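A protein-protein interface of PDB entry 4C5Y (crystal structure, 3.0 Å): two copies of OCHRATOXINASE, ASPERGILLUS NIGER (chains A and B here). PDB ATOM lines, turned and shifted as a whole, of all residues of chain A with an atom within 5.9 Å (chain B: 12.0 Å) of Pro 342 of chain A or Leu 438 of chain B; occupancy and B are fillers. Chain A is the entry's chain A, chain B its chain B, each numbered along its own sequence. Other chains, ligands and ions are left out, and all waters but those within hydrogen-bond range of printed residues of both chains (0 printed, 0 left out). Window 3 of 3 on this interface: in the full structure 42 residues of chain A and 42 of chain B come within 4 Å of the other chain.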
ATOM      1  N   SER A 289      11.947 -33.900  13.583  1.00  0.00           N
ATOM      2  CA  SER A 289      13.311 -34.174  13.105  1.00  0.00           C
ATOM      3  C   SER A 289      14.211 -34.692  14.204  1.00  0.00           C
ATOM      4  O   SER A 289      14.826 -35.736  14.057  1.00  0.00           O
ATOM      5  CB  SER A 289      13.950 -32.929  12.483  1.00  0.00           C
ATOM      6  OG  SER A 289      13.396 -32.657  11.212  1.00  0.00           O
ATOM      7  N   ILE A 293      16.052 -38.236  13.976  1.00  0.00           N
ATOM      8  CA  ILE A 293      17.507 -38.152  13.759  1.00  0.00           C
ATOM      9  C   ILE A 293      18.234 -39.025  14.776  1.00  0.00           C
ATOM     10  O   ILE A 293      19.220 -39.696  14.445  1.00  0.00           O
ATOM     11  CB  ILE A 293      18.073 -36.695  13.835  1.00  0.00           C
ATOM     12  CG1 ILE A 293      17.611 -35.846  12.641  1.00  0.00           C
ATOM     13  CG2 ILE A 293      19.604 -36.687  13.862  1.00  0.00           C
ATOM     14  CD1 ILE A 293      17.685 -34.344  12.874  1.00  0.00           C
ATOM     15  N   THR A 335      12.419 -27.650  12.930  1.00  0.00           N
ATOM     16  CA  THR A 335      13.448 -28.672  12.971  1.00  0.00           C
ATOM     17  C   THR A 335      14.179 -28.790  14.304  1.00  0.00           C
ATOM     18  O   THR A 335      14.629 -29.878  14.663  1.00  0.00           O
ATOM     19  CB  THR A 335      14.519 -28.371  11.920  1.00  0.00           C
ATOM     20  OG1 THR A 335      13.887 -28.232  10.651  1.00  0.00           O
ATOM     21  CG2 THR A 335      15.536 -29.481  11.854  1.00  0.00           C
ATOM     22  N   THR A 337      17.236 -27.117  15.062  1.00  0.00           N
ATOM     23  CA  THR A 337      18.673 -27.196  14.764  1.00  0.00           C
ATOM     24  C   THR A 337      19.254 -25.808  14.538  1.00  0.00           C
ATOM     25  O   THR A 337      18.519 -24.829  14.474  1.00  0.00           O
ATOM     26  CB  THR A 337      18.988 -28.012  13.490  1.00  0.00           C
ATOM     27  OG1 THR A 337      18.096 -27.622  12.434  1.00  0.00           O
ATOM     28  CG2 THR A 337      18.921 -29.532  13.759  1.00  0.00           C
ATOM     29  N   ALA A 338      20.581 -25.750  14.426  1.00  0.00           N
ATOM     30  CA  ALA A 338      21.281 -24.530  14.055  1.00  0.00           C
ATOM     31  C   ALA A 338      20.889 -24.049  12.655  1.00  0.00           C
ATOM     32  O   ALA A 338      20.382 -24.824  11.834  1.00  0.00           O
ATOM     33  CB  ALA A 338      22.781 -24.750  14.111  1.00  0.00           C
ATOM     34  N   GLY A 340      21.319 -23.368   8.884  1.00  0.00           N
ATOM     35  CA  GLY A 340      22.051 -24.213   7.925  1.00  0.00           C
ATOM     36  C   GLY A 340      21.868 -25.710   8.117  1.00  0.00           C
ATOM     37  O   GLY A 340      22.214 -26.505   7.253  1.00  0.00           O
ATOM     38  N   GLY A 341      21.317 -26.095   9.257  1.00  0.00           N
ATOM     39  CA  GLY A 341      20.981 -27.478   9.508  1.00  0.00           C
ATOM     40  C   GLY A 341      19.918 -28.024   8.563  1.00  0.00           C
ATOM     41  O   GLY A 341      19.349 -27.288   7.744  1.00  0.00           O
ATOM     42  N   PRO A 342      19.634 -29.324   8.693  1.00  0.00           N
ATOM     43  CA  PRO A 342      18.734 -30.042   7.819  1.00  0.00           C
ATOM     44  C   PRO A 342      17.265 -29.766   8.120  1.00  0.00           C
ATOM     45  O   PRO A 342      16.524 -30.666   8.531  1.00  0.00           O
ATOM     46  CB  PRO A 342      19.071 -31.490   8.123  1.00  0.00           C
ATOM     47  CG  PRO A 342      19.387 -31.461   9.569  1.00  0.00           C
ATOM     48  CD  PRO A 342      20.146 -30.192   9.768  1.00  0.00           C
ATOM     49  N   THR A 343      16.836 -28.542   7.860  1.00  0.00           N
ATOM     50  CA  THR A 343      15.434 -28.207   8.005  1.00  0.00           C
ATOM     51  C   THR A 343      14.554 -28.960   7.020  1.00  0.00           C
ATOM     52  O   THR A 343      13.443 -29.356   7.363  1.00  0.00           O
ATOM     53  CB  THR A 343      15.190 -26.706   7.816  1.00  0.00           C
ATOM     54  OG1 THR A 343      15.831 -26.254   6.625  1.00  0.00           O
ATOM     55  CG2 THR A 343      15.761 -25.943   8.970  1.00  0.00           C
ATOM     56  N   ALA A 344      15.042 -29.166   5.797  1.00  0.00           N
ATOM     57  CA  ALA A 344      14.268 -29.863   4.748  1.00  0.00           C
ATOM     58  C   ALA A 344      13.673 -31.211   5.190  1.00  0.00           C
ATOM     59  O   ALA A 344      12.632 -31.634   4.693  1.00  0.00           O
ATOM     60  CB  ALA A 344      15.149 -30.068   3.535  1.00  0.00           C
ATOM     61  N   LEU A 345      14.343 -31.872   6.126  1.00  0.00           N
ATOM     62  CA  LEU A 345      13.895 -33.158   6.652  1.00  0.00           C
ATOM     63  C   LEU A 345      12.499 -33.118   7.235  1.00  0.00           C
ATOM     64  O   LEU A 345      11.732 -34.066   7.093  1.00  0.00           O
ATOM     65  CB  LEU A 345      14.848 -33.638   7.759  1.00  0.00           C
ATOM     66  CG  LEU A 345      16.175 -34.308   7.450  1.00  0.00           C
ATOM     67  CD1 LEU A 345      16.726 -35.021   8.677  1.00  0.00           C
ATOM     68  CD2 LEU A 345      15.998 -35.273   6.313  1.00  0.00           C
ATOM     69  N   GLU A 346      12.180 -32.025   7.919  1.00  0.00           N
ATOM     70  CA  GLU A 346      10.935 -31.933   8.680  1.00  0.00           C
ATOM     71  C   GLU A 346       9.761 -32.140   7.733  1.00  0.00           C
ATOM     72  O   GLU A 346       8.771 -32.785   8.091  1.00  0.00           O
ATOM     73  CB  GLU A 346      10.858 -30.593   9.420  1.00  0.00           C
ATOM     74  CG  GLU A 346       9.689 -30.438  10.362  1.00  0.00           C
ATOM     75  CD  GLU A 346       9.682 -31.470  11.468  1.00  0.00           C
ATOM     76  OE1 GLU A 346      10.766 -31.823  11.980  1.00  0.00           O
ATOM     77  OE2 GLU A 346       8.578 -31.926  11.816  1.00  0.00           O
ATOM     78  N   ASP B 128      37.859 -24.448  12.531  1.00  0.00           N
ATOM     79  CA  ASP B 128      37.062 -25.672  12.427  1.00  0.00           C
ATOM     80  C   ASP B 128      36.396 -25.729  11.073  1.00  0.00           C
ATOM     81  O   ASP B 128      35.684 -26.672  10.781  1.00  0.00           O
ATOM     82  CB  ASP B 128      36.043 -25.829  13.566  1.00  0.00           C
ATOM     83  CG  ASP B 128      35.035 -24.698  13.630  1.00  0.00           C
ATOM     84  OD1 ASP B 128      35.044 -23.842  12.720  1.00  0.00           O
ATOM     85  OD2 ASP B 128      34.228 -24.653  14.598  1.00  0.00           O
ATOM     86  N   GLY B 129      36.633 -24.705  10.256  1.00  0.00           N
ATOM     87  CA  GLY B 129      36.162 -24.672   8.883  1.00  0.00           C
ATOM     88  C   GLY B 129      34.690 -24.356   8.763  1.00  0.00           C
ATOM     89  O   GLY B 129      34.061 -24.672   7.766  1.00  0.00           O
ATOM     90  N   THR B 130      34.124 -23.732   9.780  1.00  0.00           N
ATOM     91  CA  THR B 130      32.728 -23.323   9.722  1.00  0.00           C
ATOM     92  C   THR B 130      32.611 -22.108   8.803  1.00  0.00           C
ATOM     93  O   THR B 130      31.572 -21.861   8.217  1.00  0.00           O
ATOM     94  CB  THR B 130      32.184 -22.991  11.120  1.00  0.00           C
ATOM     95  OG1 THR B 130      32.179 -24.174  11.930  1.00  0.00           O
ATOM     96  CG2 THR B 130      30.789 -22.517  10.999  1.00  0.00           C
ATOM     97  N   TRP B 429      32.973 -20.931  -0.620  1.00  0.00           N
ATOM     98  CA  TRP B 429      33.613 -21.356   0.621  1.00  0.00           C
ATOM     99  C   TRP B 429      34.783 -22.253   0.309  1.00  0.00           C
ATOM    100  O   TRP B 429      35.200 -23.068   1.130  1.00  0.00           O
ATOM    101  CB  TRP B 429      32.583 -22.076   1.517  1.00  0.00           C
ATOM    102  CG  TRP B 429      31.400 -21.231   1.755  1.00  0.00           C
ATOM    103  CD1 TRP B 429      30.170 -21.338   1.168  1.00  0.00           C
ATOM    104  CD2 TRP B 429      31.343 -20.093   2.608  1.00  0.00           C
ATOM    105  NE1 TRP B 429      29.343 -20.346   1.624  1.00  0.00           N
ATOM    106  CE2 TRP B 429      30.033 -19.562   2.507  1.00  0.00           C
ATOM    107  CE3 TRP B 429      32.264 -19.481   3.470  1.00  0.00           C
ATOM    108  CZ2 TRP B 429      29.619 -18.440   3.241  1.00  0.00           C
ATOM    109  CZ3 TRP B 429      31.864 -18.367   4.185  1.00  0.00           C
ATOM    110  CH2 TRP B 429      30.547 -17.854   4.067  1.00  0.00           C
ATOM    111  N   ASP B 432      35.937 -28.359  -2.324  1.00  0.00           N
ATOM    112  CA  ASP B 432      35.407 -29.515  -1.619  1.00  0.00           C
ATOM    113  C   ASP B 432      34.603 -29.044  -0.427  1.00  0.00           C
ATOM    114  O   ASP B 432      34.547 -29.715   0.597  1.00  0.00           O
ATOM    115  CB  ASP B 432      36.549 -30.459  -1.202  1.00  0.00           C
ATOM    116  CG  ASP B 432      37.387 -30.941  -2.399  1.00  0.00           C
ATOM    117  OD1 ASP B 432      36.803 -31.262  -3.471  1.00  0.00           O
ATOM    118  OD2 ASP B 432      38.635 -31.022  -2.260  1.00  0.00           O
ATOM    119  N   ALA B 433      33.988 -27.877  -0.570  1.00  0.00           N
ATOM    120  CA  ALA B 433      33.255 -27.283   0.520  1.00  0.00           C
ATOM    121  C   ALA B 433      31.989 -28.095   0.780  1.00  0.00           C
ATOM    122  O   ALA B 433      31.402 -28.648  -0.151  1.00  0.00           O
ATOM    123  CB  ALA B 433      32.918 -25.847   0.193  1.00  0.00           C
ATOM    124  N   ARG B 434      31.618 -28.205   2.050  1.00  0.00           N
ATOM    125  CA  ARG B 434      30.396 -28.888   2.472  1.00  0.00           C
ATOM    126  C   ARG B 434      29.792 -28.120   3.633  1.00  0.00           C
ATOM    127  O   ARG B 434      30.497 -27.588   4.480  1.00  0.00           O
ATOM    128  CB  ARG B 434      30.662 -30.333   2.895  1.00  0.00           C
ATOM    129  CG  ARG B 434      30.587 -31.361   1.754  1.00  0.00           C
ATOM    130  CD  ARG B 434      31.722 -32.408   1.759  1.00  0.00           C
ATOM    131  NE  ARG B 434      32.121 -32.863   3.105  1.00  0.00           N
ATOM    132  CZ  ARG B 434      33.134 -32.376   3.852  1.00  0.00           C
ATOM    133  NH1 ARG B 434      33.913 -31.370   3.429  1.00  0.00           N
ATOM    134  NH2 ARG B 434      33.372 -32.899   5.058  1.00  0.00           N
ATOM    135  N   ASN B 435      28.475 -28.048   3.634  1.00  0.00           N
ATOM    136  CA  ASN B 435      27.739 -27.426   4.705  1.00  0.00           C
ATOM    137  C   ASN B 435      28.091 -28.090   6.029  1.00  0.00           C
ATOM    138  O   ASN B 435      27.767 -29.260   6.246  1.00  0.00           O
ATOM    139  CB  ASN B 435      26.245 -27.564   4.427  1.00  0.00           C
ATOM    140  CG  ASN B 435      25.394 -27.010   5.531  1.00  0.00           C
ATOM    141  OD1 ASN B 435      25.894 -26.609   6.572  1.00  0.00           O
ATOM    142  ND2 ASN B 435      24.096 -26.978   5.307  1.00  0.00           N
ATOM    143  N   PRO B 436      28.761 -27.344   6.923  1.00  0.00           N
ATOM    144  CA  PRO B 436      29.135 -27.911   8.212  1.00  0.00           C
ATOM    145  C   PRO B 436      27.966 -28.206   9.147  1.00  0.00           C
ATOM    146  O   PRO B 436      28.164 -28.878  10.131  1.00  0.00           O
ATOM    147  CB  PRO B 436      30.079 -26.862   8.810  1.00  0.00           C
ATOM    148  CG  PRO B 436      29.790 -25.610   8.084  1.00  0.00           C
ATOM    149  CD  PRO B 436      29.365 -26.017   6.711  1.00  0.00           C
ATOM    150  N   PHE B 437      26.758 -27.757   8.842  1.00  0.00           N
ATOM    151  CA  PHE B 437      25.625 -27.976   9.740  1.00  0.00           C
ATOM    152  C   PHE B 437      24.738 -29.161   9.362  1.00  0.00           C
ATOM    153  O   PHE B 437      23.580 -29.207   9.755  1.00  0.00           O
ATOM    154  CB  PHE B 437      24.795 -26.694   9.807  1.00  0.00           C
ATOM    155  CG  PHE B 437      25.571 -25.492  10.295  1.00  0.00           C
ATOM    156  CD1 PHE B 437      26.290 -24.706   9.414  1.00  0.00           C
ATOM    157  CD2 PHE B 437      25.577 -25.145  11.637  1.00  0.00           C
ATOM    158  CE1 PHE B 437      26.997 -23.604   9.863  1.00  0.00           C
ATOM    159  CE2 PHE B 437      26.281 -24.044  12.093  1.00  0.00           C
ATOM    160  CZ  PHE B 437      26.994 -23.277  11.204  1.00  0.00           C
ATOM    161  N   LEU B 438      25.287 -30.121   8.621  1.00  0.00           N
ATOM    162  CA  LEU B 438      24.556 -31.326   8.208  1.00  0.00           C
ATOM    163  C   LEU B 438      25.288 -32.619   8.594  1.00  0.00           C
ATOM    164  O   LEU B 438      24.696 -33.618   9.009  1.00  0.00           O
ATOM    165  CB  LEU B 438      24.342 -31.296   6.692  1.00  0.00           C
ATOM    166  CG  LEU B 438      23.468 -30.151   6.161  1.00  0.00           C
ATOM    167  CD1 LEU B 438      23.509 -30.053   4.645  1.00  0.00           C
ATOM    168  CD2 LEU B 438      22.027 -30.315   6.625  1.00  0.00           C
ATOM    169  OXT LEU B 438      26.509 -32.699   8.481  1.00  0.00           O
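OD1 of Asn 435 of chain B sits at hydrogen-bond distance from N of Phe 437 of chain B (2.7 Å).
No residue of chain B comes within 4 Å of Thr 335 of chain A.
No residue of chain B comes within 4 Å of Thr 337 of chain A.
Of chain B, only Phe 437 (3.8 Å) comes within 4 Å of Ala 338 of chain A.
Of chain B, only Asn 435, Phe 437 and Leu 438 come within 4 Å of Gly 340 of chain A.
Gly 341 of chain A touches two residues of chain B.
Of the printed residues of chain B, Pro 342 of chain A touches Phe 437 and Leu 438.
Thr 343 of chain A touches none of the printed residues of chain B.
Ala 344 of chain A touches none of the printed residues of chain B.
No residue of chain B comes within 4 Å of Leu 345 of chain A.
Of the printed residues of chain A, Asn 435 of chain B touches Gly 340 (2.7 Å).
Printed residues of chain A within 4 Å of Phe 437 of chain B: Ala 338 (3.8 Å), Gly 340 (3.5 Å), Gly 341 (3.1 Å) and Pro 342 (3.6 Å).
Leu 438 of chain B touches three residues of chain A.
The nearest residue of chain B that does not touch Pro 342 of chain A is Asn 435 of chain B (6.1 Å).
The nearest residue of chain A that does not touch Leu 438 of chain B is Thr 343 of chain A (5.6 Å).
The nearest printed residue of chain A that does not touch Asn 435 of chain B is Gly 341 of chain A (4.9 Å).
Hydrophobic or aromatic side chains of chain A that line the printed part of chain B: Ala 338 and Pro 342.
Printed residues of chain B that touch a printed residue of chain A: Asn 435, Phe 437 and Leu 438.
Among the printed residues, 8 pairs touch across the chains.
Ala 338 of chain A touches Phe 437 of chain B (CB to CD2, 3.8 Å).
C of Gly 340 of chain A touches CB of Phe 437 of chain B, at 3.5 Å.
Gly 340 of chain A touches Leu 438 of chain B.
Gly 341 of chain A touches Phe 437 of chain B (CA to O, 3.1 Å).
Leu 438 of chain B touches Gly 341 of chain A (CD2 to C, 3.7 Å).
CD of Pro 342 of chain A touches O of Phe 437 of chain B (3.6 Å).
Pro 342 of chain A touches Leu 438 of chain B.
No position is printed for both chains.
ND2 of Asn 435 of chain B sits at hydrogen-bond distance from O of Gly 340 of chain A (2.7 Å).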
